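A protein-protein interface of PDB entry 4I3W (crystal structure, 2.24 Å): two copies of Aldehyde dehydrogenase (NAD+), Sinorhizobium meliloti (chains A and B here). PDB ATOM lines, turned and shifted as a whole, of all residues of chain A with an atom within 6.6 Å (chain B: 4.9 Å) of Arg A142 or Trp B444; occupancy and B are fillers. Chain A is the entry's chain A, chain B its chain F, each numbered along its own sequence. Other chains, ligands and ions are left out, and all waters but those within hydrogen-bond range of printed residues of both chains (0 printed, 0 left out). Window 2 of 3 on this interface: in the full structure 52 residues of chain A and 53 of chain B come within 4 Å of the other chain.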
ATOM      1  N   PHE A 131      19.295  -3.964 -18.022  1.00  0.00           N
ATOM      2  CA  PHE A 131      18.529  -3.944 -16.788  1.00  0.00           C
ATOM      3  C   PHE A 131      18.248  -2.499 -16.422  1.00  0.00           C
ATOM      4  O   PHE A 131      19.132  -1.649 -16.518  1.00  0.00           O
ATOM      5  CB  PHE A 131      19.335  -4.595 -15.644  1.00  0.00           C
ATOM      6  CG  PHE A 131      19.562  -6.084 -15.816  1.00  0.00           C
ATOM      7  CD1 PHE A 131      18.700  -7.019 -15.227  1.00  0.00           C
ATOM      8  CD2 PHE A 131      20.642  -6.549 -16.536  1.00  0.00           C
ATOM      9  CE1 PHE A 131      18.940  -8.408 -15.368  1.00  0.00           C
ATOM     10  CE2 PHE A 131      20.874  -7.911 -16.684  1.00  0.00           C
ATOM     11  CZ  PHE A 131      20.021  -8.844 -16.108  1.00  0.00           C
ATOM     12  N   SER A 132      17.028  -2.222 -15.976  1.00  0.00           N
ATOM     13  CA  SER A 132      16.721  -0.916 -15.400  1.00  0.00           C
ATOM     14  C   SER A 132      16.923  -1.019 -13.898  1.00  0.00           C
ATOM     15  O   SER A 132      16.588  -2.068 -13.284  1.00  0.00           O
ATOM     16  CB  SER A 132      15.282  -0.534 -15.685  1.00  0.00           C
ATOM     17  OG  SER A 132      15.159  -0.206 -17.054  1.00  0.00           O
ATOM     18  N   CYS A 133      17.459   0.051 -13.293  1.00  0.00           N
ATOM     19  CA  CYS A 133      17.902  -0.050 -11.908  1.00  0.00           C
ATOM     20  C   CYS A 133      16.948   0.557 -10.879  1.00  0.00           C
ATOM     21  O   CYS A 133      17.235   0.531  -9.686  1.00  0.00           O
ATOM     22  CB  CYS A 133      19.304   0.550 -11.747  1.00  0.00           C
ATOM     23  SG  CYS A 133      20.560  -0.323 -12.715  1.00  0.00           S
ATOM     24  N   ASP A 134      15.829   1.106 -11.335  1.00  0.00           N
ATOM     25  CA  ASP A 134      14.920   1.870 -10.460  1.00  0.00           C
ATOM     26  C   ASP A 134      13.848   0.892  -9.958  1.00  0.00           C
ATOM     27  O   ASP A 134      12.621   1.134 -10.046  1.00  0.00           O
ATOM     28  CB  ASP A 134      14.291   3.095 -11.214  1.00  0.00           C
ATOM     29  CG  ASP A 134      13.572   2.680 -12.532  1.00  0.00           C
ATOM     30  OD1 ASP A 134      14.102   1.790 -13.256  1.00  0.00           O
ATOM     31  OD2 ASP A 134      12.475   3.214 -12.866  1.00  0.00           O
ATOM     32  N   LYS A 140      18.099   3.255  -8.531  1.00  0.00           N
ATOM     33  CA  LYS A 140      18.782   4.412  -9.121  1.00  0.00           C
ATOM     34  C   LYS A 140      18.335   4.588 -10.564  1.00  0.00           C
ATOM     35  O   LYS A 140      17.976   3.591 -11.237  1.00  0.00           O
ATOM     36  CB  LYS A 140      20.306   4.244  -9.027  1.00  0.00           C
ATOM     37  CG  LYS A 140      20.850   4.465  -7.581  1.00  0.00           C
ATOM     38  CD  LYS A 140      22.368   4.557  -7.541  1.00  0.00           C
ATOM     39  CE  LYS A 140      22.897   4.578  -6.099  1.00  0.00           C
ATOM     40  NZ  LYS A 140      22.286   5.691  -5.298  1.00  0.00           N
ATOM     41  N   ALA A 141      18.311   5.832 -11.040  1.00  0.00           N
ATOM     42  CA  ALA A 141      18.018   6.124 -12.456  1.00  0.00           C
ATOM     43  C   ALA A 141      19.235   5.781 -13.266  1.00  0.00           C
ATOM     44  O   ALA A 141      20.108   6.644 -13.514  1.00  0.00           O
ATOM     45  CB  ALA A 141      17.659   7.603 -12.658  1.00  0.00           C
ATOM     46  N   ARG A 142      19.302   4.512 -13.682  1.00  0.00           N
ATOM     47  CA  ARG A 142      20.534   3.980 -14.257  1.00  0.00           C
ATOM     48  C   ARG A 142      20.230   2.729 -15.084  1.00  0.00           C
ATOM     49  O   ARG A 142      19.234   2.035 -14.834  1.00  0.00           O
ATOM     50  CB  ARG A 142      21.499   3.672 -13.071  1.00  0.00           C
ATOM     51  CG  ARG A 142      22.778   2.900 -13.392  1.00  0.00           C
ATOM     52  CD  ARG A 142      23.754   3.018 -12.170  1.00  0.00           C
ATOM     53  NE  ARG A 142      24.232   4.395 -11.989  1.00  0.00           N
ATOM     54  CZ  ARG A 142      25.346   4.869 -12.544  1.00  0.00           C
ATOM     55  NH1 ARG A 142      26.135   4.085 -13.273  1.00  0.00           N
ATOM     56  NH2 ARG A 142      25.694   6.122 -12.330  1.00  0.00           N
ATOM     57  N   LYS A 143      21.066   2.435 -16.069  1.00  0.00           N
ATOM     58  CA  LYS A 143      20.872   1.206 -16.807  1.00  0.00           C
ATOM     59  C   LYS A 143      22.114   0.351 -16.719  1.00  0.00           C
ATOM     60  O   LYS A 143      23.232   0.884 -16.665  1.00  0.00           O
ATOM     61  CB  LYS A 143      20.478   1.480 -18.266  1.00  0.00           C
ATOM     62  CG  LYS A 143      19.006   1.872 -18.466  1.00  0.00           C
ATOM     63  CD  LYS A 143      18.730   2.239 -19.960  1.00  0.00           C
ATOM     64  CE  LYS A 143      17.276   2.701 -20.184  1.00  0.00           C
ATOM     65  NZ  LYS A 143      16.302   1.555 -20.092  1.00  0.00           N
ATOM     66  N   ILE A 144      21.925  -0.969 -16.668  1.00  0.00           N
ATOM     67  CA  ILE A 144      23.054  -1.896 -16.727  1.00  0.00           C
ATOM     68  C   ILE A 144      22.958  -2.641 -18.053  1.00  0.00           C
ATOM     69  O   ILE A 144      21.886  -3.046 -18.467  1.00  0.00           O
ATOM     70  CB  ILE A 144      23.021  -2.903 -15.574  1.00  0.00           C
ATOM     71  CG1 ILE A 144      23.205  -2.187 -14.219  1.00  0.00           C
ATOM     72  CG2 ILE A 144      24.103  -3.976 -15.786  1.00  0.00           C
ATOM     73  CD1 ILE A 144      22.839  -3.100 -13.017  1.00  0.00           C
ATOM     74  N   PHE A 145      24.081  -2.801 -18.724  1.00  0.00           N
ATOM     75  CA  PHE A 145      24.151  -3.462 -19.998  1.00  0.00           C
ATOM     76  C   PHE A 145      25.209  -4.556 -19.887  1.00  0.00           C
ATOM     77  O   PHE A 145      26.192  -4.423 -19.113  1.00  0.00           O
ATOM     78  CB  PHE A 145      24.651  -2.478 -21.055  1.00  0.00           C
ATOM     79  CG  PHE A 145      23.846  -1.209 -21.160  1.00  0.00           C
ATOM     80  CD1 PHE A 145      24.122  -0.125 -20.335  1.00  0.00           C
ATOM     81  CD2 PHE A 145      22.876  -1.071 -22.144  1.00  0.00           C
ATOM     82  CE1 PHE A 145      23.398   1.068 -20.443  1.00  0.00           C
ATOM     83  CE2 PHE A 145      22.149   0.125 -22.265  1.00  0.00           C
ATOM     84  CZ  PHE A 145      22.423   1.190 -21.419  1.00  0.00           C
ATOM     85  N   PHE A 483      28.211  -3.176 -17.598  1.00  0.00           N
ATOM     86  CA  PHE A 483      28.583  -1.759 -17.399  1.00  0.00           C
ATOM     87  C   PHE A 483      27.311  -1.014 -17.158  1.00  0.00           C
ATOM     88  O   PHE A 483      26.253  -1.366 -17.686  1.00  0.00           O
ATOM     89  CB  PHE A 483      29.439  -1.150 -18.560  1.00  0.00           C
ATOM     90  CG  PHE A 483      28.748  -1.126 -19.918  1.00  0.00           C
ATOM     91  CD1 PHE A 483      28.818  -2.228 -20.768  1.00  0.00           C
ATOM     92  CD2 PHE A 483      28.086   0.016 -20.364  1.00  0.00           C
ATOM     93  CE1 PHE A 483      28.224  -2.209 -22.015  1.00  0.00           C
ATOM     94  CE2 PHE A 483      27.477   0.037 -21.625  1.00  0.00           C
ATOM     95  CZ  PHE A 483      27.569  -1.084 -22.445  1.00  0.00           C
ATOM     96  N   SER A 484      27.367  -0.008 -16.305  1.00  0.00           N
ATOM     97  CA  SER A 484      26.172   0.784 -16.086  1.00  0.00           C
ATOM     98  C   SER A 484      26.412   2.258 -16.423  1.00  0.00           C
ATOM     99  O   SER A 484      27.520   2.785 -16.245  1.00  0.00           O
ATOM    100  CB  SER A 484      25.677   0.638 -14.639  1.00  0.00           C
ATOM    101  OG  SER A 484      26.550   1.310 -13.760  1.00  0.00           O
ATOM    102  N   LEU A 485      25.353   2.911 -16.906  1.00  0.00           N
ATOM    103  CA  LEU A 485      25.401   4.323 -17.274  1.00  0.00           C
ATOM    104  C   LEU A 485      24.310   5.086 -16.551  1.00  0.00           C
ATOM    105  O   LEU A 485      23.190   4.568 -16.378  1.00  0.00           O
ATOM    106  CB  LEU A 485      25.184   4.489 -18.773  1.00  0.00           C
ATOM    107  CG  LEU A 485      26.166   3.753 -19.675  1.00  0.00           C
ATOM    108  CD1 LEU A 485      25.719   3.943 -21.123  1.00  0.00           C
ATOM    109  CD2 LEU A 485      27.584   4.270 -19.473  1.00  0.00           C
ATOM    110  N   PRO A 486      24.612   6.325 -16.127  1.00  0.00           N
ATOM    111  CA  PRO A 486      23.550   7.191 -15.584  1.00  0.00           C
ATOM    112  C   PRO A 486      22.447   7.306 -16.607  1.00  0.00           C
ATOM    113  O   PRO A 486      22.730   7.415 -17.818  1.00  0.00           O
ATOM    114  CB  PRO A 486      24.232   8.567 -15.451  1.00  0.00           C
ATOM    115  CG  PRO A 486      25.687   8.235 -15.358  1.00  0.00           C
ATOM    116  CD  PRO A 486      25.887   7.033 -16.267  1.00  0.00           C
ATOM    117  N   TRP A 487      21.203   7.242 -16.170  1.00  0.00           N
ATOM    118  CA  TRP A 487      20.088   7.355 -17.107  1.00  0.00           C
ATOM    119  C   TRP A 487      18.953   8.229 -16.561  1.00  0.00           C
ATOM    120  O   TRP A 487      17.880   7.731 -16.163  1.00  0.00           O
ATOM    121  CB  TRP A 487      19.563   5.968 -17.519  1.00  0.00           C
ATOM    122  CG  TRP A 487      18.913   5.984 -18.908  1.00  0.00           C
ATOM    123  CD1 TRP A 487      17.599   6.175 -19.190  1.00  0.00           C
ATOM    124  CD2 TRP A 487      19.590   5.883 -20.188  1.00  0.00           C
ATOM    125  NE1 TRP A 487      17.402   6.191 -20.563  1.00  0.00           N
ATOM    126  CE2 TRP A 487      18.609   6.008 -21.192  1.00  0.00           C
ATOM    127  CE3 TRP A 487      20.931   5.717 -20.574  1.00  0.00           C
ATOM    128  CZ2 TRP A 487      18.920   5.935 -22.556  1.00  0.00           C
ATOM    129  CZ3 TRP A 487      21.241   5.664 -21.936  1.00  0.00           C
ATOM    130  CH2 TRP A 487      20.241   5.757 -22.905  1.00  0.00           C
ATOM    131  N   LEU B 270      36.719  16.556 -15.332  1.00  0.00           N
ATOM    132  CA  LEU B 270      35.651  16.950 -14.408  1.00  0.00           C
ATOM    133  C   LEU B 270      35.773  18.400 -13.933  1.00  0.00           C
ATOM    134  O   LEU B 270      36.881  18.913 -13.701  1.00  0.00           O
ATOM    135  CB  LEU B 270      35.605  16.027 -13.190  1.00  0.00           C
ATOM    136  CG  LEU B 270      35.263  14.556 -13.494  1.00  0.00           C
ATOM    137  CD1 LEU B 270      35.173  13.732 -12.176  1.00  0.00           C
ATOM    138  CD2 LEU B 270      33.935  14.523 -14.268  1.00  0.00           C
ATOM    139  N   ASP B 274      31.838  18.621 -10.106  1.00  0.00           N
ATOM    140  CA  ASP B 274      31.845  17.182 -10.339  1.00  0.00           C
ATOM    141  C   ASP B 274      32.874  16.493  -9.445  1.00  0.00           C
ATOM    142  O   ASP B 274      32.623  15.401  -8.914  1.00  0.00           O
ATOM    143  CB  ASP B 274      32.086  16.845 -11.816  1.00  0.00           C
ATOM    144  CG  ASP B 274      30.850  17.040 -12.675  1.00  0.00           C
ATOM    145  OD1 ASP B 274      29.705  16.942 -12.159  1.00  0.00           O
ATOM    146  OD2 ASP B 274      31.025  17.277 -13.890  1.00  0.00           O
ATOM    147  N   ARG B 277      31.171  15.727  -6.305  1.00  0.00           N
ATOM    148  CA  ARG B 277      30.284  14.572  -6.349  1.00  0.00           C
ATOM    149  C   ARG B 277      31.107  13.295  -6.344  1.00  0.00           C
ATOM    150  O   ARG B 277      30.735  12.330  -5.681  1.00  0.00           O
ATOM    151  CB  ARG B 277      29.366  14.618  -7.574  1.00  0.00           C
ATOM    152  CG  ARG B 277      28.688  15.976  -7.753  1.00  0.00           C
ATOM    153  CD  ARG B 277      27.336  15.881  -8.503  1.00  0.00           C
ATOM    154  NE  ARG B 277      27.449  15.531  -9.928  1.00  0.00           N
ATOM    155  CZ  ARG B 277      27.300  14.295 -10.415  1.00  0.00           C
ATOM    156  NH1 ARG B 277      27.044  13.280  -9.591  1.00  0.00           N
ATOM    157  NH2 ARG B 277      27.406  14.062 -11.724  1.00  0.00           N
ATOM    158  N   ALA B 278      32.241  13.319  -7.045  1.00  0.00           N
ATOM    159  CA  ALA B 278      33.166  12.191  -7.065  1.00  0.00           C
ATOM    160  C   ALA B 278      33.765  11.946  -5.680  1.00  0.00           C
ATOM    161  O   ALA B 278      34.002  10.791  -5.279  1.00  0.00           O
ATOM    162  CB  ALA B 278      34.300  12.422  -8.108  1.00  0.00           C
ATOM    163  N   LEU B 281      31.443   9.990  -3.642  1.00  0.00           N
ATOM    164  CA  LEU B 281      31.414   8.589  -4.022  1.00  0.00           C
ATOM    165  C   LEU B 281      32.644   7.929  -3.439  1.00  0.00           C
ATOM    166  O   LEU B 281      32.538   6.840  -2.889  1.00  0.00           O
ATOM    167  CB  LEU B 281      31.399   8.434  -5.549  1.00  0.00           C
ATOM    168  CG  LEU B 281      30.070   8.804  -6.234  1.00  0.00           C
ATOM    169  CD1 LEU B 281      30.203   8.659  -7.716  1.00  0.00           C
ATOM    170  CD2 LEU B 281      28.916   7.926  -5.729  1.00  0.00           C
ATOM    171  N   VAL B 421      34.038   4.744 -12.630  1.00  0.00           N
ATOM    172  CA  VAL B 421      34.771   5.742 -13.407  1.00  0.00           C
ATOM    173  C   VAL B 421      33.948   7.024 -13.425  1.00  0.00           C
ATOM    174  O   VAL B 421      32.746   7.004 -13.761  1.00  0.00           O
ATOM    175  CB  VAL B 421      35.004   5.298 -14.850  1.00  0.00           C
ATOM    176  CG1 VAL B 421      35.870   6.333 -15.585  1.00  0.00           C
ATOM    177  CG2 VAL B 421      35.696   3.941 -14.935  1.00  0.00           C
ATOM    178  N   CYS B 422      34.567   8.136 -13.028  1.00  0.00           N
ATOM    179  CA  CYS B 422      33.864   9.438 -13.037  1.00  0.00           C
ATOM    180  C   CYS B 422      34.389  10.335 -14.166  1.00  0.00           C
ATOM    181  O   CYS B 422      35.566  10.738 -14.165  1.00  0.00           O
ATOM    182  CB  CYS B 422      34.025  10.142 -11.701  1.00  0.00           C
ATOM    183  SG  CYS B 422      33.343   9.217 -10.344  1.00  0.00           S
ATOM    184  N   THR B 423      33.520  10.619 -15.139  1.00  0.00           N
ATOM    185  CA  THR B 423      33.912  11.394 -16.317  1.00  0.00           C
ATOM    186  C   THR B 423      32.643  11.750 -17.053  1.00  0.00           C
ATOM    187  O   THR B 423      31.602  11.140 -16.813  1.00  0.00           O
ATOM    188  CB  THR B 423      34.807  10.588 -17.250  1.00  0.00           C
ATOM    189  OG1 THR B 423      35.219  11.408 -18.358  1.00  0.00           O
ATOM    190  CG2 THR B 423      34.053   9.351 -17.800  1.00  0.00           C
ATOM    191  N   ASN B 424      32.709  12.763 -17.918  1.00  0.00           N
ATOM    192  CA  ASN B 424      31.550  13.138 -18.721  1.00  0.00           C
ATOM    193  C   ASN B 424      31.815  12.970 -20.202  1.00  0.00           C
ATOM    194  O   ASN B 424      30.954  13.233 -21.050  1.00  0.00           O
ATOM    195  CB  ASN B 424      31.116  14.587 -18.421  1.00  0.00           C
ATOM    196  CG  ASN B 424      30.756  14.786 -16.966  1.00  0.00           C
ATOM    197  OD1 ASN B 424      29.995  13.991 -16.380  1.00  0.00           O
ATOM    198  ND2 ASN B 424      31.318  15.836 -16.359  1.00  0.00           N
ATOM    199  N   ASN B 442      31.094   0.657 -13.494  1.00  0.00           N
ATOM    200  CA  ASN B 442      30.006   1.598 -13.238  1.00  0.00           C
ATOM    201  C   ASN B 442      30.436   3.025 -13.589  1.00  0.00           C
ATOM    202  O   ASN B 442      31.459   3.533 -13.088  1.00  0.00           O
ATOM    203  CB  ASN B 442      29.550   1.543 -11.777  1.00  0.00           C
ATOM    204  CG  ASN B 442      28.888   0.221 -11.422  1.00  0.00           C
ATOM    205  OD1 ASN B 442      28.102  -0.326 -12.203  1.00  0.00           O
ATOM    206  ND2 ASN B 442      29.170  -0.280 -10.215  1.00  0.00           N
ATOM    207  N   ILE B 443      29.655   3.697 -14.430  1.00  0.00           N
ATOM    208  CA  ILE B 443      29.988   5.082 -14.745  1.00  0.00           C
ATOM    209  C   ILE B 443      29.304   5.994 -13.729  1.00  0.00           C
ATOM    210  O   ILE B 443      28.069   5.954 -13.567  1.00  0.00           O
ATOM    211  CB  ILE B 443      29.585   5.476 -16.173  1.00  0.00           C
ATOM    212  CG1 ILE B 443      30.295   4.604 -17.194  1.00  0.00           C
ATOM    213  CG2 ILE B 443      29.915   6.957 -16.453  1.00  0.00           C
ATOM    214  CD1 ILE B 443      31.833   4.635 -17.093  1.00  0.00           C
ATOM    215  N   TRP B 444      30.100   6.814 -13.042  1.00  0.00           N
ATOM    216  CA  TRP B 444      29.552   7.719 -12.038  1.00  0.00           C
ATOM    217  C   TRP B 444      28.810   6.976 -10.931  1.00  0.00           C
ATOM    218  O   TRP B 444      27.785   7.455 -10.450  1.00  0.00           O
ATOM    219  CB  TRP B 444      28.618   8.751 -12.684  1.00  0.00           C
ATOM    220  CG  TRP B 444      29.330  10.001 -13.057  1.00  0.00           C
ATOM    221  CD1 TRP B 444      29.532  10.509 -14.332  1.00  0.00           C
ATOM    222  CD2 TRP B 444      29.940  10.933 -12.157  1.00  0.00           C
ATOM    223  NE1 TRP B 444      30.229  11.708 -14.258  1.00  0.00           N
ATOM    224  CE2 TRP B 444      30.495  11.982 -12.939  1.00  0.00           C
ATOM    225  CE3 TRP B 444      30.054  10.997 -10.765  1.00  0.00           C
ATOM    226  CZ2 TRP B 444      31.184  13.059 -12.368  1.00  0.00           C
ATOM    227  CZ3 TRP B 444      30.740  12.077 -10.192  1.00  0.00           C
ATOM    228  CH2 TRP B 444      31.301  13.088 -10.998  1.00  0.00           C
ATOM    229  N   GLU B 445      29.315   5.803 -10.526  1.00  0.00           N
ATOM    230  CA  GLU B 445      28.839   5.164  -9.300  1.00  0.00           C
ATOM    231  C   GLU B 445      30.010   4.409  -8.684  1.00  0.00           C
ATOM    232  O   GLU B 445      31.044   4.269  -9.355  1.00  0.00           O
ATOM    233  CB  GLU B 445      27.661   4.235  -9.581  1.00  0.00           C
ATOM    234  CG  GLU B 445      26.350   4.758  -9.065  1.00  0.00           C
ATOM    235  CD  GLU B 445      26.361   4.922  -7.529  1.00  0.00           C
ATOM    236  OE1 GLU B 445      27.359   4.510  -6.877  1.00  0.00           O
ATOM    237  OE2 GLU B 445      25.380   5.486  -6.970  1.00  0.00           O
ATOM    238  N   VAL B 446      29.893   3.980  -7.424  1.00  0.00           N
ATOM    239  CA  VAL B 446      30.991   3.217  -6.804  1.00  0.00           C
ATOM    240  C   VAL B 446      31.059   1.849  -7.467  1.00  0.00           C
ATOM    241  O   VAL B 446      30.116   1.448  -8.134  1.00  0.00           O
ATOM    242  CB  VAL B 446      30.827   3.102  -5.296  1.00  0.00           C
ATOM    243  CG1 VAL B 446      30.988   4.526  -4.647  1.00  0.00           C
ATOM    244  CG2 VAL B 446      29.464   2.533  -4.955  1.00  0.00           C
ATOM    245  N   TYR B 449      28.223  -0.584  -6.608  1.00  0.00           N
ATOM    246  CA  TYR B 449      26.817  -0.514  -7.033  1.00  0.00           C
ATOM    247  C   TYR B 449      26.359  -1.675  -7.955  1.00  0.00           C
ATOM    248  O   TYR B 449      26.988  -1.961  -8.998  1.00  0.00           O
ATOM    249  CB  TYR B 449      26.482   0.841  -7.697  1.00  0.00           C
ATOM    250  CG  TYR B 449      25.038   0.811  -8.100  1.00  0.00           C
ATOM    251  CD1 TYR B 449      24.035   1.015  -7.139  1.00  0.00           C
ATOM    252  CD2 TYR B 449      24.658   0.465  -9.400  1.00  0.00           C
ATOM    253  CE1 TYR B 449      22.680   0.933  -7.461  1.00  0.00           C
ATOM    254  CE2 TYR B 449      23.286   0.373  -9.749  1.00  0.00           C
ATOM    255  CZ  TYR B 449      22.309   0.609  -8.767  1.00  0.00           C
ATOM    256  OH  TYR B 449      20.968   0.549  -9.082  1.00  0.00           O
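Printed residues of chain B within 4 Å of Arg A142: Ile B443 (2.7 Å), Trp B444 (3.1 Å), Glu B445 (3.6 Å) and Tyr B449 (3.6 Å).
Printed residues of chain A within 4 Å of Glu B445: Lys A140 (2.8 Å) and Arg A142 (3.6 Å).
Of the printed residues of chain A, Tyr B449 touches Cys A133, Lys A140 and Arg A142.
Of the printed residues of chain B, Ser A484 touches Asn B442 and Ile B443.
Of the printed residues of chain B, Pro A486 touches Ile B443 (3.6 Å).
The nearest printed residue of chain A that does not touch Trp B444 is Pro A486 (4.001 Å).
The nearest printed residue of chain B that does not touch Pro A486 is Trp B444 (4.001 Å).
No position is printed for both chains.
Hydrophobic or aromatic side chains of chain B within 4 Å of the printed part of chain A: Ile B443, Trp B444 and Tyr B449.
Along chain B the printed residues that touch a printed residue of chain A span positions 442 to 449.
Of the 15 printed residues of chain A, 6 touch a printed residue of chain B.
Printed residues of chain A that touch a printed residue of chain B: Cys A133, Lys A140, Arg A142, Ser A484, Leu A485 and Pro A486.
Among the printed residues, 11 pairs touch across the chains.
Lys A140 touches Tyr B449.
Arg A142 touches Glu B445 (NH2 to CG, 3.6 Å).
Arg A142 touches Tyr B449.
Ile B443 touches Leu A485.
CD of Pro A486 touches O of Ile B443 (3.6 Å).
O of Ile B443 lies within hydrogen-bond range of NH2 of Arg A142 (2.7 Å).
The side-chain hydroxyl (OH) of Tyr B449 lies close to the side-chain sulfur (SG) of Cys A133, at 3.8 Å.
O of Ser A484 sits at hydrogen-bond distance from N of Ile B443, 2.9 Å away.
The side-chain carboxylate (OE2) of Glu B445 is in salt-bridge range of the side-chain amino group (NZ) of Lys A140.
The side-chain amide oxygen of Asn B442 lies within hydrogen-bond range of the side-chain hydroxyl of Ser A484.
The guanidinium group of Arg A142 lies within hydrogen-bond range of the backbone carbonyl oxygen of Trp B444 (3.1 Å).
N of Asp A134 sits at hydrogen-bond distance from O of Lys A140 (3.3 Å).
OG of Ser A484 is in hydrogen-bond range of NH1 of Arg A142.
The backbone NH (N) of Cys A133 sits at hydrogen-bond distance from the backbone carbonyl oxygen (O) of Arg A142, at 3.1 Å.
O of Asn B442 lies within hydrogen-bond range of N of Val B421, at 2.9 Å.
The backbone NH (N) of Leu A485 lies within hydrogen-bond range of the backbone carbonyl oxygen (O) of Lys A143.
The side-chain amide nitrogen (ND2) of Asn B442 lies within hydrogen-bond range of the backbone carbonyl oxygen (O) of Tyr B449 (3.0 Å).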
